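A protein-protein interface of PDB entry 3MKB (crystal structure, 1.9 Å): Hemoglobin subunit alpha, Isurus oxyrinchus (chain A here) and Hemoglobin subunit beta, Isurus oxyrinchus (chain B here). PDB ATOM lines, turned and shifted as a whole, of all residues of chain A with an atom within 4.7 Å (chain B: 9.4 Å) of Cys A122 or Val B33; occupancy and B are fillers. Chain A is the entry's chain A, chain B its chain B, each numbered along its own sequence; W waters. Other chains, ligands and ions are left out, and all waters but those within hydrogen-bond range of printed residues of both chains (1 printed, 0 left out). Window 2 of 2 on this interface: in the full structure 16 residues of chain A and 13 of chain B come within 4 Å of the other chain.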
ATOM      1  N   GLU A   6     -14.647 -18.355   0.840  1.00  0.00           N
ATOM      2  CA  GLU A   6     -13.375 -17.729   0.507  1.00  0.00           C
ATOM      3  C   GLU A   6     -13.298 -17.340  -0.957  1.00  0.00           C
ATOM      4  O   GLU A   6     -12.831 -16.247  -1.269  1.00  0.00           O
ATOM      5  CB  GLU A   6     -12.220 -18.626   0.921  1.00  0.00           C
ATOM      6  CG  GLU A   6     -11.989 -18.540   2.440  1.00  0.00           C
ATOM      7  CD  GLU A   6     -11.121 -19.632   2.953  1.00  0.00           C
ATOM      8  OE1 GLU A   6     -10.993 -20.650   2.235  1.00  0.00           O
ATOM      9  OE2 GLU A   6     -10.601 -19.482   4.082  1.00  0.00           O
ATOM     10  N   PRO A 118     -11.426 -10.847  10.043  1.00  0.00           N
ATOM     11  CA  PRO A 118     -10.575 -12.000  10.131  1.00  0.00           C
ATOM     12  C   PRO A 118     -10.877 -13.075   9.061  1.00  0.00           C
ATOM     13  O   PRO A 118      -9.934 -13.666   8.553  1.00  0.00           O
ATOM     14  CB  PRO A 118     -10.825 -12.509  11.550  1.00  0.00           C
ATOM     15  CG  PRO A 118     -11.214 -11.329  12.292  1.00  0.00           C
ATOM     16  CD  PRO A 118     -12.029 -10.519  11.360  1.00  0.00           C
ATOM     17  N   ALA A 119     -12.153 -13.338   8.762  1.00  0.00           N
ATOM     18  CA  ALA A 119     -12.463 -14.287   7.685  1.00  0.00           C
ATOM     19  C   ALA A 119     -11.917 -13.842   6.306  1.00  0.00           C
ATOM     20  O   ALA A 119     -11.369 -14.645   5.556  1.00  0.00           O
ATOM     21  CB  ALA A 119     -14.021 -14.597   7.630  1.00  0.00           C
ATOM     22  N   THR A 120     -12.034 -12.568   6.001  1.00  0.00           N
ATOM     23  CA  THR A 120     -11.602 -12.013   4.702  1.00  0.00           C
ATOM     24  C   THR A 120     -10.071 -12.067   4.568  1.00  0.00           C
ATOM     25  O   THR A 120      -9.511 -12.526   3.587  1.00  0.00           O
ATOM     26  CB  THR A 120     -12.058 -10.535   4.595  1.00  0.00           C
ATOM     27  OG1 THR A 120     -13.480 -10.519   4.481  1.00  0.00           O
ATOM     28  CG2 THR A 120     -11.436  -9.829   3.380  1.00  0.00           C
ATOM     29  N   HIS A 121      -9.413 -11.590   5.616  1.00  0.00           N
ATOM     30  CA  HIS A 121      -7.961 -11.661   5.754  1.00  0.00           C
ATOM     31  C   HIS A 121      -7.463 -13.103   5.601  1.00  0.00           C
ATOM     32  O   HIS A 121      -6.468 -13.370   4.903  1.00  0.00           O
ATOM     33  CB  HIS A 121      -7.682 -11.084   7.155  1.00  0.00           C
ATOM     34  CG  HIS A 121      -6.249 -11.118   7.579  1.00  0.00           C
ATOM     35  ND1 HIS A 121      -5.848 -10.583   8.779  1.00  0.00           N
ATOM     36  CD2 HIS A 121      -5.134 -11.627   6.999  1.00  0.00           C
ATOM     37  CE1 HIS A 121      -4.550 -10.784   8.939  1.00  0.00           C
ATOM     38  NE2 HIS A 121      -4.096 -11.416   7.874  1.00  0.00           N
ATOM     39  N   CYS A 122      -8.159 -14.038   6.252  1.00  0.00           N
ATOM     40  CA  CYS A 122      -7.780 -15.444   6.168  1.00  0.00           C
ATOM     41  C   CYS A 122      -7.845 -15.861   4.698  1.00  0.00           C
ATOM     42  O   CYS A 122      -6.902 -16.444   4.161  1.00  0.00           O
ATOM     43  CB  CYS A 122      -8.652 -16.327   7.100  1.00  0.00           C
ATOM     44  SG  CYS A 122      -8.145 -17.965   7.003  1.00  0.00           S
ATOM     45  N   ALA A 123      -8.944 -15.542   4.041  1.00  0.00           N
ATOM     46  CA  ALA A 123      -9.104 -15.868   2.602  1.00  0.00           C
ATOM     47  C   ALA A 123      -7.972 -15.347   1.707  1.00  0.00           C
ATOM     48  O   ALA A 123      -7.393 -16.101   0.887  1.00  0.00           O
ATOM     49  CB  ALA A 123     -10.406 -15.342   2.117  1.00  0.00           C
ATOM     50  N   VAL A 124      -7.667 -14.061   1.849  1.00  0.00           N
ATOM     51  CA  VAL A 124      -6.610 -13.439   1.033  1.00  0.00           C
ATOM     52  C   VAL A 124      -5.244 -14.021   1.356  1.00  0.00           C
ATOM     53  O   VAL A 124      -4.481 -14.383   0.441  1.00  0.00           O
ATOM     54  CB  VAL A 124      -6.579 -11.906   1.168  1.00  0.00           C
ATOM     55  CG1 VAL A 124      -5.602 -11.277   0.108  1.00  0.00           C
ATOM     56  CG2 VAL A 124      -7.973 -11.366   0.993  1.00  0.00           C
ATOM     57  N   ASP A 125      -4.918 -14.104   2.650  1.00  0.00           N
ATOM     58  CA  ASP A 125      -3.672 -14.728   3.068  1.00  0.00           C
ATOM     59  C   ASP A 125      -3.492 -16.127   2.507  1.00  0.00           C
ATOM     60  O   ASP A 125      -2.372 -16.499   2.140  1.00  0.00           O
ATOM     61  CB  ASP A 125      -3.534 -14.797   4.584  1.00  0.00           C
ATOM     62  CG  ASP A 125      -2.077 -14.953   5.022  1.00  0.00           C
ATOM     63  OD1 ASP A 125      -1.167 -14.491   4.295  1.00  0.00           O
ATOM     64  OD2 ASP A 125      -1.847 -15.423   6.142  1.00  0.00           O
ATOM     65  N   LYS A 126      -4.585 -16.886   2.377  1.00  0.00           N
ATOM     66  CA  LYS A 126      -4.493 -18.184   1.708  1.00  0.00           C
ATOM     67  C   LYS A 126      -4.135 -18.093   0.242  1.00  0.00           C
ATOM     68  O   LYS A 126      -3.296 -18.865  -0.224  1.00  0.00           O
ATOM     69  CB  LYS A 126      -5.774 -19.020   1.868  1.00  0.00           C
ATOM     70  CG  LYS A 126      -5.943 -19.477   3.292  1.00  0.00           C
ATOM     71  CD  LYS A 126      -7.312 -20.121   3.506  1.00  0.00           C
ATOM     72  CE  LYS A 126      -7.342 -21.506   2.852  1.00  0.00           C
ATOM     73  NZ  LYS A 126      -8.451 -22.345   3.423  1.00  0.00           N
ATOM     74  N   LYS B  26      -9.649  -7.573  19.330  1.00  0.00           N
ATOM     75  CA  LYS B  26      -9.743  -7.874  17.883  1.00  0.00           C
ATOM     76  C   LYS B  26      -8.490  -8.518  17.352  1.00  0.00           C
ATOM     77  O   LYS B  26      -8.587  -9.408  16.525  1.00  0.00           O
ATOM     78  CB  LYS B  26     -10.022  -6.625  17.053  1.00  0.00           C
ATOM     79  CG  LYS B  26     -11.234  -5.851  17.501  1.00  0.00           C
ATOM     80  CD  LYS B  26     -11.372  -4.559  16.717  1.00  0.00           C
ATOM     81  CE  LYS B  26     -12.405  -3.639  17.365  1.00  0.00           C
ATOM     82  NZ  LYS B  26     -12.571  -2.337  16.624  1.00  0.00           N
ATOM     83  N   ALA B  27      -7.305  -8.064  17.800  1.00  0.00           N
ATOM     84  CA  ALA B  27      -6.048  -8.699  17.284  1.00  0.00           C
ATOM     85  C   ALA B  27      -5.946 -10.198  17.647  1.00  0.00           C
ATOM     86  O   ALA B  27      -5.562 -11.026  16.822  1.00  0.00           O
ATOM     87  CB  ALA B  27      -4.796  -7.961  17.747  1.00  0.00           C
ATOM     88  N   LEU B  28      -6.238 -10.508  18.910  1.00  0.00           N
ATOM     89  CA  LEU B  28      -6.286 -11.865  19.400  1.00  0.00           C
ATOM     90  C   LEU B  28      -7.277 -12.714  18.582  1.00  0.00           C
ATOM     91  O   LEU B  28      -6.951 -13.862  18.161  1.00  0.00           O
ATOM     92  CB  LEU B  28      -6.685 -11.823  20.893  1.00  0.00           C
ATOM     93  CG  LEU B  28      -6.039 -12.632  22.002  1.00  0.00           C
ATOM     94  CD1 LEU B  28      -7.024 -13.695  22.566  1.00  0.00           C
ATOM     95  CD2 LEU B  28      -4.635 -13.241  21.723  1.00  0.00           C
ATOM     96  N   GLU B  29      -8.482 -12.163  18.390  1.00  0.00           N
ATOM     97  CA  GLU B  29      -9.566 -12.835  17.651  1.00  0.00           C
ATOM     98  C   GLU B  29      -9.144 -13.105  16.212  1.00  0.00           C
ATOM     99  O   GLU B  29      -9.343 -14.217  15.665  1.00  0.00           O
ATOM    100  CB  GLU B  29     -10.889 -12.018  17.714  1.00  0.00           C
ATOM    101  CG  GLU B  29     -11.547 -12.103  19.113  1.00  0.00           C
ATOM    102  CD  GLU B  29     -12.714 -11.109  19.335  1.00  0.00           C
ATOM    103  OE1 GLU B  29     -12.881 -10.129  18.544  1.00  0.00           O
ATOM    104  OE2 GLU B  29     -13.414 -11.304  20.349  1.00  0.00           O
ATOM    105  N   ARG B  30      -8.521 -12.098  15.609  1.00  0.00           N
ATOM    106  CA  ARG B  30      -7.977 -12.233  14.292  1.00  0.00           C
ATOM    107  C   ARG B  30      -6.932 -13.306  14.194  1.00  0.00           C
ATOM    108  O   ARG B  30      -6.947 -14.135  13.249  1.00  0.00           O
ATOM    109  CB  ARG B  30      -7.388 -10.886  13.821  1.00  0.00           C
ATOM    110  CG  ARG B  30      -6.777 -10.903  12.388  1.00  0.00           C
ATOM    111  CD  ARG B  30      -6.311  -9.434  11.996  1.00  0.00           C
ATOM    112  NE  ARG B  30      -7.439  -8.511  12.070  1.00  0.00           N
ATOM    113  CZ  ARG B  30      -8.287  -8.283  11.063  1.00  0.00           C
ATOM    114  NH1 ARG B  30      -8.120  -8.900   9.894  1.00  0.00           N
ATOM    115  NH2 ARG B  30      -9.305  -7.437  11.223  1.00  0.00           N
ATOM    116  N   MET B  31      -6.000 -13.289  15.146  1.00  0.00           N
ATOM    117  CA  MET B  31      -4.890 -14.253  15.143  1.00  0.00           C
ATOM    118  C   MET B  31      -5.458 -15.676  15.201  1.00  0.00           C
ATOM    119  O   MET B  31      -4.982 -16.554  14.514  1.00  0.00           O
ATOM    120  CB  MET B  31      -3.963 -14.004  16.321  1.00  0.00           C
ATOM    121  CG  MET B  31      -2.767 -14.985  16.407  1.00  0.00           C
ATOM    122  SD  MET B  31      -1.995 -14.884  18.035  1.00  0.00           S
ATOM    123  CE  MET B  31      -3.339 -15.447  19.095  1.00  0.00           C
ATOM    124  N   PHE B  32      -6.527 -15.874  15.960  1.00  0.00           N
ATOM    125  CA  PHE B  32      -7.203 -17.202  15.981  1.00  0.00           C
ATOM    126  C   PHE B  32      -7.772 -17.699  14.668  1.00  0.00           C
ATOM    127  O   PHE B  32      -7.889 -18.922  14.481  1.00  0.00           O
ATOM    128  CB  PHE B  32      -8.344 -17.224  17.007  1.00  0.00           C
ATOM    129  CG  PHE B  32      -7.890 -17.049  18.408  1.00  0.00           C
ATOM    130  CD1 PHE B  32      -6.629 -17.371  18.775  1.00  0.00           C
ATOM    131  CD2 PHE B  32      -8.771 -16.610  19.383  1.00  0.00           C
ATOM    132  CE1 PHE B  32      -6.217 -17.188  20.127  1.00  0.00           C
ATOM    133  CE2 PHE B  32      -8.377 -16.439  20.678  1.00  0.00           C
ATOM    134  CZ  PHE B  32      -7.128 -16.732  21.059  1.00  0.00           C
ATOM    135  N   VAL B  33      -8.245 -16.793  13.814  1.00  0.00           N
ATOM    136  CA  VAL B  33      -8.928 -17.147  12.571  1.00  0.00           C
ATOM    137  C   VAL B  33      -7.811 -17.263  11.549  1.00  0.00           C
ATOM    138  O   VAL B  33      -7.758 -18.244  10.783  1.00  0.00           O
ATOM    139  CB  VAL B  33     -10.002 -16.078  12.175  1.00  0.00           C
ATOM    140  CG1 VAL B  33     -10.572 -16.238  10.697  1.00  0.00           C
ATOM    141  CG2 VAL B  33     -11.158 -16.101  13.129  1.00  0.00           C
ATOM    142  N   VAL B  34      -6.894 -16.280  11.542  1.00  0.00           N
ATOM    143  CA  VAL B  34      -5.822 -16.281  10.530  1.00  0.00           C
ATOM    144  C   VAL B  34      -4.770 -17.364  10.790  1.00  0.00           C
ATOM    145  O   VAL B  34      -4.291 -17.988   9.828  1.00  0.00           O
ATOM    146  CB  VAL B  34      -5.217 -14.839  10.272  1.00  0.00           C
ATOM    147  CG1 VAL B  34      -4.052 -14.884   9.240  1.00  0.00           C
ATOM    148  CG2 VAL B  34      -6.302 -13.917   9.795  1.00  0.00           C
ATOM    149  N   PHE B  35      -4.448 -17.602  12.071  1.00  0.00           N
ATOM    150  CA  PHE B  35      -3.486 -18.619  12.519  1.00  0.00           C
ATOM    151  C   PHE B  35      -4.064 -19.552  13.604  1.00  0.00           C
ATOM    152  O   PHE B  35      -3.697 -19.448  14.772  1.00  0.00           O
ATOM    153  CB  PHE B  35      -2.187 -17.961  13.045  1.00  0.00           C
ATOM    154  CG  PHE B  35      -1.652 -16.906  12.144  1.00  0.00           C
ATOM    155  CD1 PHE B  35      -1.713 -15.551  12.524  1.00  0.00           C
ATOM    156  CD2 PHE B  35      -1.097 -17.245  10.889  1.00  0.00           C
ATOM    157  CE1 PHE B  35      -1.219 -14.547  11.684  1.00  0.00           C
ATOM    158  CE2 PHE B  35      -0.549 -16.229  10.019  1.00  0.00           C
ATOM    159  CZ  PHE B  35      -0.638 -14.893  10.409  1.00  0.00           C
ATOM    160  N   PRO B  36      -4.963 -20.498  13.219  1.00  0.00           N
ATOM    161  CA  PRO B  36      -5.769 -21.303  14.196  1.00  0.00           C
ATOM    162  C   PRO B  36      -4.971 -22.101  15.203  1.00  0.00           C
ATOM    163  O   PRO B  36      -5.430 -22.387  16.325  1.00  0.00           O
ATOM    164  CB  PRO B  36      -6.555 -22.243  13.275  1.00  0.00           C
ATOM    165  CG  PRO B  36      -6.743 -21.475  12.119  1.00  0.00           C
ATOM    166  CD  PRO B  36      -5.353 -20.857  11.858  1.00  0.00           C
ATOM    167  N   TRP B  37      -3.741 -22.444  14.834  1.00  0.00           N
ATOM    168  CA  TRP B  37      -2.975 -23.281  15.704  1.00  0.00           C
ATOM    169  C   TRP B  37      -2.670 -22.503  16.953  1.00  0.00           C
ATOM    170  O   TRP B  37      -2.394 -23.104  17.980  1.00  0.00           O
ATOM    171  CB  TRP B  37      -1.701 -23.800  15.003  1.00  0.00           C
ATOM    172  CG  TRP B  37      -0.751 -22.711  14.544  1.00  0.00           C
ATOM    173  CD1 TRP B  37       0.201 -22.138  15.274  1.00  0.00           C
ATOM    174  CD2 TRP B  37      -0.726 -22.087  13.267  1.00  0.00           C
ATOM    175  NE1 TRP B  37       0.867 -21.209  14.542  1.00  0.00           N
ATOM    176  CE2 TRP B  37       0.315 -21.163  13.286  1.00  0.00           C
ATOM    177  CE3 TRP B  37      -1.470 -22.244  12.088  1.00  0.00           C
ATOM    178  CZ2 TRP B  37       0.612 -20.362  12.216  1.00  0.00           C
ATOM    179  CZ3 TRP B  37      -1.144 -21.472  10.983  1.00  0.00           C
ATOM    180  CH2 TRP B  37      -0.101 -20.549  11.059  1.00  0.00           C
ATOM    181  N   THR B  38      -2.772 -21.173  16.887  1.00  0.00           N
ATOM    182  CA  THR B  38      -2.503 -20.315  18.063  1.00  0.00           C
ATOM    183  C   THR B  38      -3.601 -20.364  19.132  1.00  0.00           C
ATOM    184  O   THR B  38      -3.380 -19.921  20.253  1.00  0.00           O
ATOM    185  CB  THR B  38      -2.347 -18.856  17.685  1.00  0.00           C
ATOM    186  OG1 THR B  38      -3.565 -18.395  17.078  1.00  0.00           O
ATOM    187  CG2 THR B  38      -1.191 -18.692  16.716  1.00  0.00           C
ATOM    188  N   ASN B  39      -4.774 -20.883  18.780  1.00  0.00           N
ATOM    189  CA  ASN B  39      -5.834 -21.076  19.781  1.00  0.00           C
ATOM    190  C   ASN B  39      -5.555 -22.227  20.763  1.00  0.00           C
ATOM    191  O   ASN B  39      -6.269 -22.375  21.755  1.00  0.00           O
ATOM    192  CB  ASN B  39      -7.245 -21.166  19.134  1.00  0.00           C
ATOM    193  CG  ASN B  39      -8.398 -20.670  20.093  1.00  0.00           C
ATOM    194  OD1 ASN B  39      -9.445 -20.213  19.634  1.00  0.00           O
ATOM    195  ND2 ASN B  39      -8.197 -20.780  21.398  1.00  0.00           N
ATOM    196  N   LEU B  95       2.862 -13.574  15.463  1.00  0.00           N
ATOM    197  CA  LEU B  95       1.521 -13.760  14.898  1.00  0.00           C
ATOM    198  C   LEU B  95       0.531 -12.870  15.656  1.00  0.00           C
ATOM    199  O   LEU B  95      -0.376 -12.316  15.084  1.00  0.00           O
ATOM    200  CB  LEU B  95       1.120 -15.230  14.989  1.00  0.00           C
ATOM    201  CG  LEU B  95       2.122 -16.153  14.297  1.00  0.00           C
ATOM    202  CD1 LEU B  95       1.673 -17.684  14.387  1.00  0.00           C
ATOM    203  CD2 LEU B  95       2.266 -15.721  12.853  1.00  0.00           C
ATOM    204  N   SER B  99      -0.959  -9.242  14.016  1.00  0.00           N
ATOM    205  CA  SER B  99      -2.394  -9.004  14.012  1.00  0.00           C
ATOM    206  C   SER B  99      -2.719  -7.658  14.620  1.00  0.00           C
ATOM    207  O   SER B  99      -3.660  -7.052  14.246  1.00  0.00           O
ATOM    208  CB  SER B  99      -3.117 -10.078  14.827  1.00  0.00           C
ATOM    209  OG  SER B  99      -2.783 -11.365  14.377  1.00  0.00           O
ATOM    210  N   VAL B 102      -2.191  -5.203  11.996  1.00  0.00           N
ATOM    211  CA  VAL B 102      -3.376  -5.172  11.112  1.00  0.00           C
ATOM    212  C   VAL B 102      -4.493  -4.347  11.788  1.00  0.00           C
ATOM    213  O   VAL B 102      -5.172  -3.600  11.100  1.00  0.00           O
ATOM    214  CB  VAL B 102      -3.826  -6.575  10.698  1.00  0.00           C
ATOM    215  CG1 VAL B 102      -5.276  -6.573  10.021  1.00  0.00           C
ATOM    216  CG2 VAL B 102      -2.806  -7.157   9.710  1.00  0.00           C
HETATM  217  O   HOH W   1      -9.531 -19.879   9.917  1.00  0.00           O
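Pro A118 touches Arg B30 (N to NH1, 3.8 Å). Pro A118 touches Val B33. O of Pro A118 touches CG2 of Val B34 (3.8 Å). Ala A119 touches Val B33 (N to CG1, 3.8 Å). Val B34 touches His A121. Val B33 touches Cys A122. Asp A125 touches Val B34 (OD2 to CG1, 3.8 Å).
Of the printed residues of chain B, Cys A122 touches Val B33 (3.8 Å). Of chain A, only Pro A118 (3.4 Å), Ala A119 (3.8 Å) and Cys A122 (3.8 Å) come within 4 Å of Val B33. Printed residues of chain B within 4 Å of Pro A118: Arg B30 (3.8 Å), Val B33 (3.4 Å) and Val B34 (3.8 Å). Of the printed residues of chain A, Val B34 touches Pro A118, His A121 and Asp A125. Val B102 touches none of the printed residues of chain A. Phe B35 touches none of the printed residues of chain A. The nearest printed residue of chain B that does not touch Asp A125 is Phe B35 (4.2 Å).
Of the 17 printed residues of chain B, 3 touch a printed residue of chain A. Hydrophobic or aromatic side chains of chain B within 4 Å of the printed part of chain A: Val B33 and Val B34. Printed residues of chain A that touch a printed residue of chain B: Pro A118, Ala A119, His A121, Cys A122 and Asp A125. Hydrophobic or aromatic side chains of chain A that line the printed part of chain B: Pro A118 and His A121. Among the printed residues, no Asp or Glu carboxylate lies within 4 Å of a Lys or Arg side-chain nitrogen of the other chain.
Water W1 lies within hydrogen-bond range of O of Val B33 (2.6 Å) and SG of Cys A122 (3.8 Å).
ND1 of His A121 is in hydrogen-bond range of NH1 of Arg B30, 3.0 Å away.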
